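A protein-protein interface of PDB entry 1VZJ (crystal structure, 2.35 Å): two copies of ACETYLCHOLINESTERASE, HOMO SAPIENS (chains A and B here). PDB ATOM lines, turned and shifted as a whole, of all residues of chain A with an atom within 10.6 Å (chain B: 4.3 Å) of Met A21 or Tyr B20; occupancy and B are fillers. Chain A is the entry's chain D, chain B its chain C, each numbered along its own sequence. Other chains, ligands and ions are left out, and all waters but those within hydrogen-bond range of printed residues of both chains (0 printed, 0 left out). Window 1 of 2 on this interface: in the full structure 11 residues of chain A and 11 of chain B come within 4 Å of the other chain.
Met A21 touches two residues of chain B.
No residue of chain A comes within 4 Å of Arg B16.
No residue of chain A comes within 4 Å of Ser B19.
No residue of chain A comes within 4 Å of Met B21.
Printed residues of chain A within 4 Å of Trp B17: Trp A17 (3.9 Å) and Met A21 (3.7 Å).
Of the printed residues of chain B, Trp A24 touches Tyr B20 and Trp B24.
Asn A26 touches none of the printed residues of chain B.
Phe A14 touches none of the printed residues of chain B.
Trp A17 touches its own counterpart, Trp B17.
Met A21 touches Trp B17, but with the chains exchanged Trp A17 does not touch Met B21 (8.8 Å).
Trp A24 touches Tyr B20, but with the chains exchanged Tyr A20 does not touch Trp B24 (11.4 Å).
Trp B24 touches its own counterpart, Trp A24.
Positions printed for both chains: 16, 17, 18, 19, 20, 21, 22, 23 and 24.
Of the 8 pairs that touch across the chains among the printed residues, 2 have their exchanged pair printed and touching as well.
Of the 18 printed residues of chain A, 5 touch a printed residue of chain B.
Along chain A the printed residues that touch a printed residue of chain B span positions 17 to 28.
Along chain B the printed residues that touch a printed residue of chain A span positions 17 to 24.
Among the printed residues, 8 pairs touch across the chains.
Among the printed residues, merely in contact across the chains: Trp A24 with Tyr B20 (3.3 Å), Met A21 with Tyr B20 (3.4 Å), Lys A25 with Tyr B20 (3.5 Å), Met A21 with Trp B17 (3.7 Å), Trp A24 with Trp B24 (3.7 Å), Phe A28 with Trp B24 (3.8 Å), Phe A28 with His B23 (3.9 Å) and Trp A17 with Trp B17 (3.9 Å).
NZ of Lys A25 is in salt-bridge range of OD2 of Asp A29, at 3.2 Å.
O of Phe A28 lies within hydrogen-bond range of OG of Ser A32.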
ATOM      1  N   GLU A  13     -33.932   2.990  17.068  1.00  0.00           N
ATOM      2  CA  GLU A  13     -32.640   3.343  17.652  1.00  0.00           C
ATOM      3  C   GLU A  13     -31.758   2.122  17.920  1.00  0.00           C
ATOM      4  O   GLU A  13     -30.534   2.199  17.795  1.00  0.00           O
ATOM      5  CB  GLU A  13     -32.827   4.141  18.942  1.00  0.00           C
ATOM      6  CG  GLU A  13     -33.464   5.489  18.714  1.00  0.00           C
ATOM      7  CD  GLU A  13     -33.468   6.363  19.948  1.00  0.00           C
ATOM      8  OE1 GLU A  13     -34.039   5.963  20.993  1.00  0.00           O
ATOM      9  OE2 GLU A  13     -32.899   7.470  19.863  1.00  0.00           O
ATOM     10  N   PHE A  14     -32.389   1.007  18.283  1.00  0.00           N
ATOM     11  CA  PHE A  14     -31.680  -0.238  18.558  1.00  0.00           C
ATOM     12  C   PHE A  14     -30.920  -0.633  17.309  1.00  0.00           C
ATOM     13  O   PHE A  14     -29.687  -0.672  17.287  1.00  0.00           O
ATOM     14  CB  PHE A  14     -32.682  -1.338  18.887  1.00  0.00           C
ATOM     15  CG  PHE A  14     -32.058  -2.623  19.352  1.00  0.00           C
ATOM     16  CD1 PHE A  14     -32.547  -3.848  18.896  1.00  0.00           C
ATOM     17  CD2 PHE A  14     -31.048  -2.621  20.305  1.00  0.00           C
ATOM     18  CE1 PHE A  14     -32.048  -5.050  19.395  1.00  0.00           C
ATOM     19  CE2 PHE A  14     -30.541  -3.815  20.809  1.00  0.00           C
ATOM     20  CZ  PHE A  14     -31.037  -5.029  20.359  1.00  0.00           C
ATOM     21  N   HIS A  15     -31.688  -0.944  16.274  1.00  0.00           N
ATOM     22  CA  HIS A  15     -31.161  -1.338  14.983  1.00  0.00           C
ATOM     23  C   HIS A  15     -30.100  -0.368  14.462  1.00  0.00           C
ATOM     24  O   HIS A  15     -29.127  -0.781  13.845  1.00  0.00           O
ATOM     25  CB  HIS A  15     -32.324  -1.466  13.982  1.00  0.00           C
ATOM     26  CG  HIS A  15     -33.178  -2.680  14.200  1.00  0.00           C
ATOM     27  ND1 HIS A  15     -34.378  -2.865  13.538  1.00  0.00           N
ATOM     28  CD2 HIS A  15     -32.992  -3.771  14.966  1.00  0.00           C
ATOM     29  CE1 HIS A  15     -34.888  -4.030  13.896  1.00  0.00           C
ATOM     30  NE2 HIS A  15     -34.072  -4.602  14.760  1.00  0.00           N
ATOM     31  N   ARG A  16     -30.276   0.916  14.724  1.00  0.00           N
ATOM     32  CA  ARG A  16     -29.311   1.894  14.268  1.00  0.00           C
ATOM     33  C   ARG A  16     -28.045   1.731  15.085  1.00  0.00           C
ATOM     34  O   ARG A  16     -26.935   1.929  14.597  1.00  0.00           O
ATOM     35  CB  ARG A  16     -29.865   3.304  14.433  1.00  0.00           C
ATOM     36  CG  ARG A  16     -28.986   4.396  13.856  1.00  0.00           C
ATOM     37  CD  ARG A  16     -29.660   5.764  13.975  1.00  0.00           C
ATOM     38  NE  ARG A  16     -29.132   6.711  12.995  1.00  0.00           N
ATOM     39  CZ  ARG A  16     -28.409   7.789  13.291  1.00  0.00           C
ATOM     40  NH1 ARG A  16     -28.112   8.085  14.554  1.00  0.00           N
ATOM     41  NH2 ARG A  16     -27.977   8.571  12.309  1.00  0.00           N
ATOM     42  N   TRP A  17     -28.227   1.363  16.346  1.00  0.00           N
ATOM     43  CA  TRP A  17     -27.112   1.136  17.253  1.00  0.00           C
ATOM     44  C   TRP A  17     -26.410  -0.143  16.821  1.00  0.00           C
ATOM     45  O   TRP A  17     -25.181  -0.175  16.691  1.00  0.00           O
ATOM     46  CB  TRP A  17     -27.626   0.981  18.680  1.00  0.00           C
ATOM     47  CG  TRP A  17     -26.570   0.626  19.669  1.00  0.00           C
ATOM     48  CD1 TRP A  17     -25.636   1.454  20.180  1.00  0.00           C
ATOM     49  CD2 TRP A  17     -26.357  -0.652  20.271  1.00  0.00           C
ATOM     50  NE1 TRP A  17     -24.851   0.783  21.072  1.00  0.00           N
ATOM     51  CE2 TRP A  17     -25.275  -0.516  21.149  1.00  0.00           C
ATOM     52  CE3 TRP A  17     -26.983  -1.895  20.155  1.00  0.00           C
ATOM     53  CZ2 TRP A  17     -24.792  -1.583  21.923  1.00  0.00           C
ATOM     54  CZ3 TRP A  17     -26.509  -2.956  20.919  1.00  0.00           C
ATOM     55  CH2 TRP A  17     -25.423  -2.790  21.797  1.00  0.00           C
ATOM     56  N   SER A  18     -27.194  -1.195  16.603  1.00  0.00           N
ATOM     57  CA  SER A  18     -26.633  -2.464  16.155  1.00  0.00           C
ATOM     58  C   SER A  18     -25.796  -2.284  14.908  1.00  0.00           C
ATOM     59  O   SER A  18     -24.941  -3.113  14.605  1.00  0.00           O
ATOM     60  CB  SER A  18     -27.722  -3.475  15.830  1.00  0.00           C
ATOM     61  OG  SER A  18     -28.193  -4.110  16.996  1.00  0.00           O
ATOM     62  N   SER A  19     -26.043  -1.203  14.180  1.00  0.00           N
ATOM     63  CA  SER A  19     -25.300  -0.980  12.958  1.00  0.00           C
ATOM     64  C   SER A  19     -23.988  -0.275  13.198  1.00  0.00           C
ATOM     65  O   SER A  19     -23.084  -0.347  12.372  1.00  0.00           O
ATOM     66  CB  SER A  19     -26.130  -0.197  11.962  1.00  0.00           C
ATOM     67  OG  SER A  19     -26.082  -0.880  10.726  1.00  0.00           O
ATOM     68  N   TYR A  20     -23.894   0.428  14.316  1.00  0.00           N
ATOM     69  CA  TYR A  20     -22.660   1.106  14.659  1.00  0.00           C
ATOM     70  C   TYR A  20     -21.812   0.026  15.303  1.00  0.00           C
ATOM     71  O   TYR A  20     -20.587   0.112  15.342  1.00  0.00           O
ATOM     72  CB  TYR A  20     -22.914   2.218  15.669  1.00  0.00           C
ATOM     73  CG  TYR A  20     -23.242   3.556  15.069  1.00  0.00           C
ATOM     74  CD1 TYR A  20     -24.562   3.930  14.812  1.00  0.00           C
ATOM     75  CD2 TYR A  20     -22.230   4.466  14.787  1.00  0.00           C
ATOM     76  CE1 TYR A  20     -24.867   5.195  14.290  1.00  0.00           C
ATOM     77  CE2 TYR A  20     -22.513   5.723  14.270  1.00  0.00           C
ATOM     78  CZ  TYR A  20     -23.830   6.089  14.026  1.00  0.00           C
ATOM     79  OH  TYR A  20     -24.097   7.369  13.567  1.00  0.00           O
ATOM     80  N   MET A  21     -22.483  -0.996  15.820  1.00  0.00           N
ATOM     81  CA  MET A  21     -21.790  -2.099  16.453  1.00  0.00           C
ATOM     82  C   MET A  21     -21.024  -2.825  15.354  1.00  0.00           C
ATOM     83  O   MET A  21     -19.814  -3.001  15.441  1.00  0.00           O
ATOM     84  CB  MET A  21     -22.799  -3.040  17.125  1.00  0.00           C
ATOM     85  CG  MET A  21     -22.202  -3.988  18.192  1.00  0.00           C
ATOM     86  SD  MET A  21     -21.959  -3.224  19.976  1.00  0.00           S
ATOM     87  CE  MET A  21     -20.721  -1.937  19.551  1.00  0.00           C
ATOM     88  N   VAL A  22     -21.731  -3.222  14.300  1.00  0.00           N
ATOM     89  CA  VAL A  22     -21.114  -3.918  13.180  1.00  0.00           C
ATOM     90  C   VAL A  22     -20.022  -3.069  12.557  1.00  0.00           C
ATOM     91  O   VAL A  22     -18.956  -3.560  12.200  1.00  0.00           O
ATOM     92  CB  VAL A  22     -22.137  -4.260  12.084  1.00  0.00           C
ATOM     93  CG1 VAL A  22     -21.429  -4.899  10.903  1.00  0.00           C
ATOM     94  CG2 VAL A  22     -23.184  -5.235  12.617  1.00  0.00           C
ATOM     95  N   HIS A  23     -20.275  -1.785  12.429  1.00  0.00           N
ATOM     96  CA  HIS A  23     -19.281  -0.930  11.832  1.00  0.00           C
ATOM     97  C   HIS A  23     -18.049  -0.807  12.716  1.00  0.00           C
ATOM     98  O   HIS A  23     -16.921  -0.677  12.214  1.00  0.00           O
ATOM     99  CB  HIS A  23     -19.843   0.464  11.560  1.00  0.00           C
ATOM    100  CG  HIS A  23     -18.898   1.333  10.795  1.00  0.00           C
ATOM    101  ND1 HIS A  23     -18.555   2.607  11.194  1.00  0.00           N
ATOM    102  CD2 HIS A  23     -18.195   1.090   9.659  1.00  0.00           C
ATOM    103  CE1 HIS A  23     -17.685   3.113  10.337  1.00  0.00           C
ATOM    104  NE2 HIS A  23     -17.450   2.213   9.397  1.00  0.00           N
ATOM    105  N   TRP A  24     -18.262  -0.819  14.034  1.00  0.00           N
ATOM    106  CA  TRP A  24     -17.154  -0.702  14.964  1.00  0.00           C
ATOM    107  C   TRP A  24     -16.395  -2.020  15.003  1.00  0.00           C
ATOM    108  O   TRP A  24     -15.168  -2.032  15.058  1.00  0.00           O
ATOM    109  CB  TRP A  24     -17.653  -0.360  16.366  1.00  0.00           C
ATOM    110  CG  TRP A  24     -16.577  -0.444  17.390  1.00  0.00           C
ATOM    111  CD1 TRP A  24     -15.770   0.557  17.795  1.00  0.00           C
ATOM    112  CD2 TRP A  24     -16.126  -1.626  18.066  1.00  0.00           C
ATOM    113  NE1 TRP A  24     -14.832   0.085  18.679  1.00  0.00           N
ATOM    114  CE2 TRP A  24     -15.029  -1.257  18.861  1.00  0.00           C
ATOM    115  CE3 TRP A  24     -16.540  -2.960  18.067  1.00  0.00           C
ATOM    116  CZ2 TRP A  24     -14.331  -2.176  19.660  1.00  0.00           C
ATOM    117  CZ3 TRP A  24     -15.847  -3.878  18.862  1.00  0.00           C
ATOM    118  CH2 TRP A  24     -14.755  -3.479  19.645  1.00  0.00           C
ATOM    119  N   LYS A  25     -17.123  -3.131  14.982  1.00  0.00           N
ATOM    120  CA  LYS A  25     -16.475  -4.435  15.019  1.00  0.00           C
ATOM    121  C   LYS A  25     -15.512  -4.538  13.857  1.00  0.00           C
ATOM    122  O   LYS A  25     -14.394  -5.034  13.993  1.00  0.00           O
ATOM    123  CB  LYS A  25     -17.495  -5.556  14.902  1.00  0.00           C
ATOM    124  CG  LYS A  25     -16.845  -6.914  14.920  1.00  0.00           C
ATOM    125  CD  LYS A  25     -16.053  -7.121  16.228  1.00  0.00           C
ATOM    126  CE  LYS A  25     -15.169  -8.374  16.166  1.00  0.00           C
ATOM    127  NZ  LYS A  25     -15.935  -9.561  15.716  1.00  0.00           N
ATOM    128  N   ASN A  26     -15.976  -4.051  12.714  1.00  0.00           N
ATOM    129  CA  ASN A  26     -15.232  -4.051  11.465  1.00  0.00           C
ATOM    130  C   ASN A  26     -13.935  -3.266  11.553  1.00  0.00           C
ATOM    131  O   ASN A  26     -12.879  -3.730  11.143  1.00  0.00           O
ATOM    132  CB  ASN A  26     -16.098  -3.440  10.369  1.00  0.00           C
ATOM    133  CG  ASN A  26     -16.094  -4.255   9.113  1.00  0.00           C
ATOM    134  OD1 ASN A  26     -16.697  -5.328   9.059  1.00  0.00           O
ATOM    135  ND2 ASN A  26     -15.413  -3.758   8.088  1.00  0.00           N
ATOM    136  N   GLN A  27     -14.034  -2.053  12.061  1.00  0.00           N
ATOM    137  CA  GLN A  27     -12.871  -1.207  12.193  1.00  0.00           C
ATOM    138  C   GLN A  27     -11.907  -1.832  13.191  1.00  0.00           C
ATOM    139  O   GLN A  27     -10.688  -1.758  13.024  1.00  0.00           O
ATOM    140  CB  GLN A  27     -13.299   0.185  12.658  1.00  0.00           C
ATOM    141  CG  GLN A  27     -14.076   0.994  11.617  1.00  0.00           C
ATOM    142  CD  GLN A  27     -13.182   1.628  10.550  1.00  0.00           C
ATOM    143  OE1 GLN A  27     -13.605   2.551   9.848  1.00  0.00           O
ATOM    144  NE2 GLN A  27     -11.951   1.136  10.418  1.00  0.00           N
ATOM    145  N   PHE A  28     -12.465  -2.467  14.215  1.00  0.00           N
ATOM    146  CA  PHE A  28     -11.674  -3.113  15.259  1.00  0.00           C
ATOM    147  C   PHE A  28     -10.867  -4.312  14.761  1.00  0.00           C
ATOM    148  O   PHE A  28      -9.675  -4.434  15.053  1.00  0.00           O
ATOM    149  CB  PHE A  28     -12.587  -3.560  16.406  1.00  0.00           C
ATOM    150  CG  PHE A  28     -11.869  -4.303  17.495  1.00  0.00           C
ATOM    151  CD1 PHE A  28     -10.978  -3.652  18.330  1.00  0.00           C
ATOM    152  CD2 PHE A  28     -12.100  -5.652  17.692  1.00  0.00           C
ATOM    153  CE1 PHE A  28     -10.315  -4.341  19.337  1.00  0.00           C
ATOM    154  CE2 PHE A  28     -11.444  -6.351  18.696  1.00  0.00           C
ATOM    155  CZ  PHE A  28     -10.554  -5.694  19.525  1.00  0.00           C
ATOM    156  N   ASP A  29     -11.516  -5.205  14.027  1.00  0.00           N
ATOM    157  CA  ASP A  29     -10.830  -6.379  13.502  1.00  0.00           C
ATOM    158  C   ASP A  29      -9.725  -6.010  12.500  1.00  0.00           C
ATOM    159  O   ASP A  29      -8.687  -6.685  12.442  1.00  0.00           O
ATOM    160  CB  ASP A  29     -11.836  -7.327  12.862  1.00  0.00           C
ATOM    161  CG  ASP A  29     -12.656  -8.065  13.885  1.00  0.00           C
ATOM    162  OD1 ASP A  29     -12.130  -8.310  14.992  1.00  0.00           O
ATOM    163  OD2 ASP A  29     -13.813  -8.420  13.582  1.00  0.00           O
ATOM    164  N   SER A  32      -6.254  -4.638  14.255  1.00  0.00           N
ATOM    165  CA  SER A  32      -5.419  -5.746  14.685  1.00  0.00           C
ATOM    166  C   SER A  32      -4.525  -6.257  13.557  1.00  0.00           C
ATOM    167  O   SER A  32      -4.972  -6.979  12.672  1.00  0.00           O
ATOM    168  CB  SER A  32      -6.329  -6.889  15.186  1.00  0.00           C
ATOM    169  OG  SER A  32      -7.428  -6.307  15.871  1.00  0.00           O
ATOM    170  N   ARG B  16     -23.185  -9.992  22.922  1.00  0.00           N
ATOM    171  CA  ARG B  16     -22.194  -9.684  21.911  1.00  0.00           C
ATOM    172  C   ARG B  16     -21.398  -8.457  22.277  1.00  0.00           C
ATOM    173  O   ARG B  16     -20.251  -8.322  21.895  1.00  0.00           O
ATOM    174  CB  ARG B  16     -22.877  -9.467  20.564  1.00  0.00           C
ATOM    175  CG  ARG B  16     -21.979  -8.849  19.532  1.00  0.00           C
ATOM    176  CD  ARG B  16     -22.730  -8.707  18.249  1.00  0.00           C
ATOM    177  NE  ARG B  16     -23.126 -10.023  17.771  1.00  0.00           N
ATOM    178  CZ  ARG B  16     -24.074 -10.236  16.872  1.00  0.00           C
ATOM    179  NH1 ARG B  16     -24.738  -9.214  16.348  1.00  0.00           N
ATOM    180  NH2 ARG B  16     -24.345 -11.475  16.488  1.00  0.00           N
ATOM    181  N   TRP B  17     -22.031  -7.544  22.995  1.00  0.00           N
ATOM    182  CA  TRP B  17     -21.380  -6.312  23.445  1.00  0.00           C
ATOM    183  C   TRP B  17     -20.320  -6.625  24.518  1.00  0.00           C
ATOM    184  O   TRP B  17     -19.240  -6.041  24.506  1.00  0.00           O
ATOM    185  CB  TRP B  17     -22.421  -5.357  24.032  1.00  0.00           C
ATOM    186  CG  TRP B  17     -21.861  -4.056  24.445  1.00  0.00           C
ATOM    187  CD1 TRP B  17     -21.576  -3.016  23.641  1.00  0.00           C
ATOM    188  CD2 TRP B  17     -21.474  -3.661  25.771  1.00  0.00           C
ATOM    189  NE1 TRP B  17     -21.029  -1.973  24.363  1.00  0.00           N
ATOM    190  CE2 TRP B  17     -20.962  -2.343  25.684  1.00  0.00           C
ATOM    191  CE3 TRP B  17     -21.515  -4.286  27.026  1.00  0.00           C
ATOM    192  CZ2 TRP B  17     -20.487  -1.633  26.800  1.00  0.00           C
ATOM    193  CZ3 TRP B  17     -21.040  -3.583  28.146  1.00  0.00           C
ATOM    194  CH2 TRP B  17     -20.538  -2.266  28.021  1.00  0.00           C
ATOM    195  N   SER B  18     -20.631  -7.530  25.443  1.00  0.00           N
ATOM    196  CA  SER B  18     -19.677  -7.886  26.491  1.00  0.00           C
ATOM    197  C   SER B  18     -18.425  -8.488  25.866  1.00  0.00           C
ATOM    198  O   SER B  18     -17.306  -8.215  26.310  1.00  0.00           O
ATOM    199  CB  SER B  18     -20.298  -8.880  27.462  1.00  0.00           C
ATOM    200  OG  SER B  18     -21.422  -8.305  28.103  1.00  0.00           O
ATOM    201  N   SER B  19     -18.630  -9.301  24.829  1.00  0.00           N
ATOM    202  CA  SER B  19     -17.545  -9.929  24.097  1.00  0.00           C
ATOM    203  C   SER B  19     -16.677  -8.856  23.460  1.00  0.00           C
ATOM    204  O   SER B  19     -15.456  -8.909  23.554  1.00  0.00           O
ATOM    205  CB  SER B  19     -18.117 -10.841  23.020  1.00  0.00           C
ATOM    206  OG  SER B  19     -17.099 -11.277  22.131  1.00  0.00           O
ATOM    207  N   TYR B  20     -17.303  -7.881  22.811  1.00  0.00           N
ATOM    208  CA  TYR B  20     -16.555  -6.798  22.193  1.00  0.00           C
ATOM    209  C   TYR B  20     -15.727  -6.085  23.249  1.00  0.00           C
ATOM    210  O   TYR B  20     -14.610  -5.640  22.989  1.00  0.00           O
ATOM    211  CB  TYR B  20     -17.496  -5.811  21.516  1.00  0.00           C
ATOM    212  CG  TYR B  20     -18.071  -6.286  20.197  1.00  0.00           C
ATOM    213  CD1 TYR B  20     -18.002  -7.626  19.808  1.00  0.00           C
ATOM    214  CD2 TYR B  20     -18.728  -5.391  19.346  1.00  0.00           C
ATOM    215  CE1 TYR B  20     -18.577  -8.057  18.608  1.00  0.00           C
ATOM    216  CE2 TYR B  20     -19.309  -5.813  18.150  1.00  0.00           C
ATOM    217  CZ  TYR B  20     -19.233  -7.145  17.788  1.00  0.00           C
ATOM    218  OH  TYR B  20     -19.843  -7.565  16.621  1.00  0.00           O
ATOM    219  N   MET B  21     -16.268  -5.987  24.451  1.00  0.00           N
ATOM    220  CA  MET B  21     -15.550  -5.358  25.546  1.00  0.00           C
ATOM    221  C   MET B  21     -14.380  -6.216  26.050  1.00  0.00           C
ATOM    222  O   MET B  21     -13.293  -5.693  26.329  1.00  0.00           O
ATOM    223  CB  MET B  21     -16.532  -5.052  26.672  1.00  0.00           C
ATOM    224  CG  MET B  21     -17.498  -3.956  26.289  1.00  0.00           C
ATOM    225  SD  MET B  21     -16.848  -2.280  26.815  1.00  0.00           S
ATOM    226  CE  MET B  21     -15.835  -1.652  25.481  1.00  0.00           C
ATOM    227  N   VAL B  22     -14.577  -7.525  26.164  1.00  0.00           N
ATOM    228  CA  VAL B  22     -13.489  -8.388  26.613  1.00  0.00           C
ATOM    229  C   VAL B  22     -12.298  -8.325  25.645  1.00  0.00           C
ATOM    230  O   VAL B  22     -11.176  -8.057  26.064  1.00  0.00           O
ATOM    231  CB  VAL B  22     -13.950  -9.842  26.735  1.00  0.00           C
ATOM    232  CG1 VAL B  22     -12.773 -10.742  27.000  1.00  0.00           C
ATOM    233  CG2 VAL B  22     -14.965  -9.963  27.845  1.00  0.00           C
ATOM    234  N   HIS B  23     -12.553  -8.571  24.360  1.00  0.00           N
ATOM    235  CA  HIS B  23     -11.534  -8.537  23.303  1.00  0.00           C
ATOM    236  C   HIS B  23     -10.907  -7.172  23.229  1.00  0.00           C
ATOM    237  O   HIS B  23      -9.699  -7.038  23.045  1.00  0.00           O
ATOM    238  CB  HIS B  23     -12.158  -8.812  21.933  1.00  0.00           C
ATOM    239  CG  HIS B  23     -12.462 -10.255  21.671  1.00  0.00           C
ATOM    240  ND1 HIS B  23     -11.505 -11.153  21.256  1.00  0.00           N
ATOM    241  CD2 HIS B  23     -13.614 -10.957  21.771  1.00  0.00           C
ATOM    242  CE1 HIS B  23     -12.052 -12.345  21.109  1.00  0.00           C
ATOM    243  NE2 HIS B  23     -13.331 -12.254  21.417  1.00  0.00           N
ATOM    244  N   TRP B  24     -11.736  -6.138  23.358  1.00  0.00           N
ATOM    245  CA  TRP B  24     -11.230  -4.786  23.275  1.00  0.00           C
ATOM    246  C   TRP B  24     -10.339  -4.419  24.441  1.00  0.00           C
ATOM    247  O   TRP B  24      -9.288  -3.833  24.234  1.00  0.00           O
ATOM    248  CB  TRP B  24     -12.355  -3.767  23.174  1.00  0.00           C
ATOM    249  CG  TRP B  24     -11.780  -2.385  23.057  1.00  0.00           C
ATOM    250  CD1 TRP B  24     -11.432  -1.735  21.906  1.00  0.00           C
ATOM    251  CD2 TRP B  24     -11.351  -1.546  24.137  1.00  0.00           C
ATOM    252  NE1 TRP B  24     -10.807  -0.549  22.202  1.00  0.00           N
ATOM    253  CE2 TRP B  24     -10.747  -0.406  23.564  1.00  0.00           C
ATOM    254  CE3 TRP B  24     -11.409  -1.654  25.530  1.00  0.00           C
ATOM    255  CZ2 TRP B  24     -10.208   0.628  24.342  1.00  0.00           C
ATOM    256  CZ3 TRP B  24     -10.868  -0.629  26.307  1.00  0.00           C
ATOM    257  CH2 TRP B  24     -10.276   0.500  25.710  1.00  0.00           C
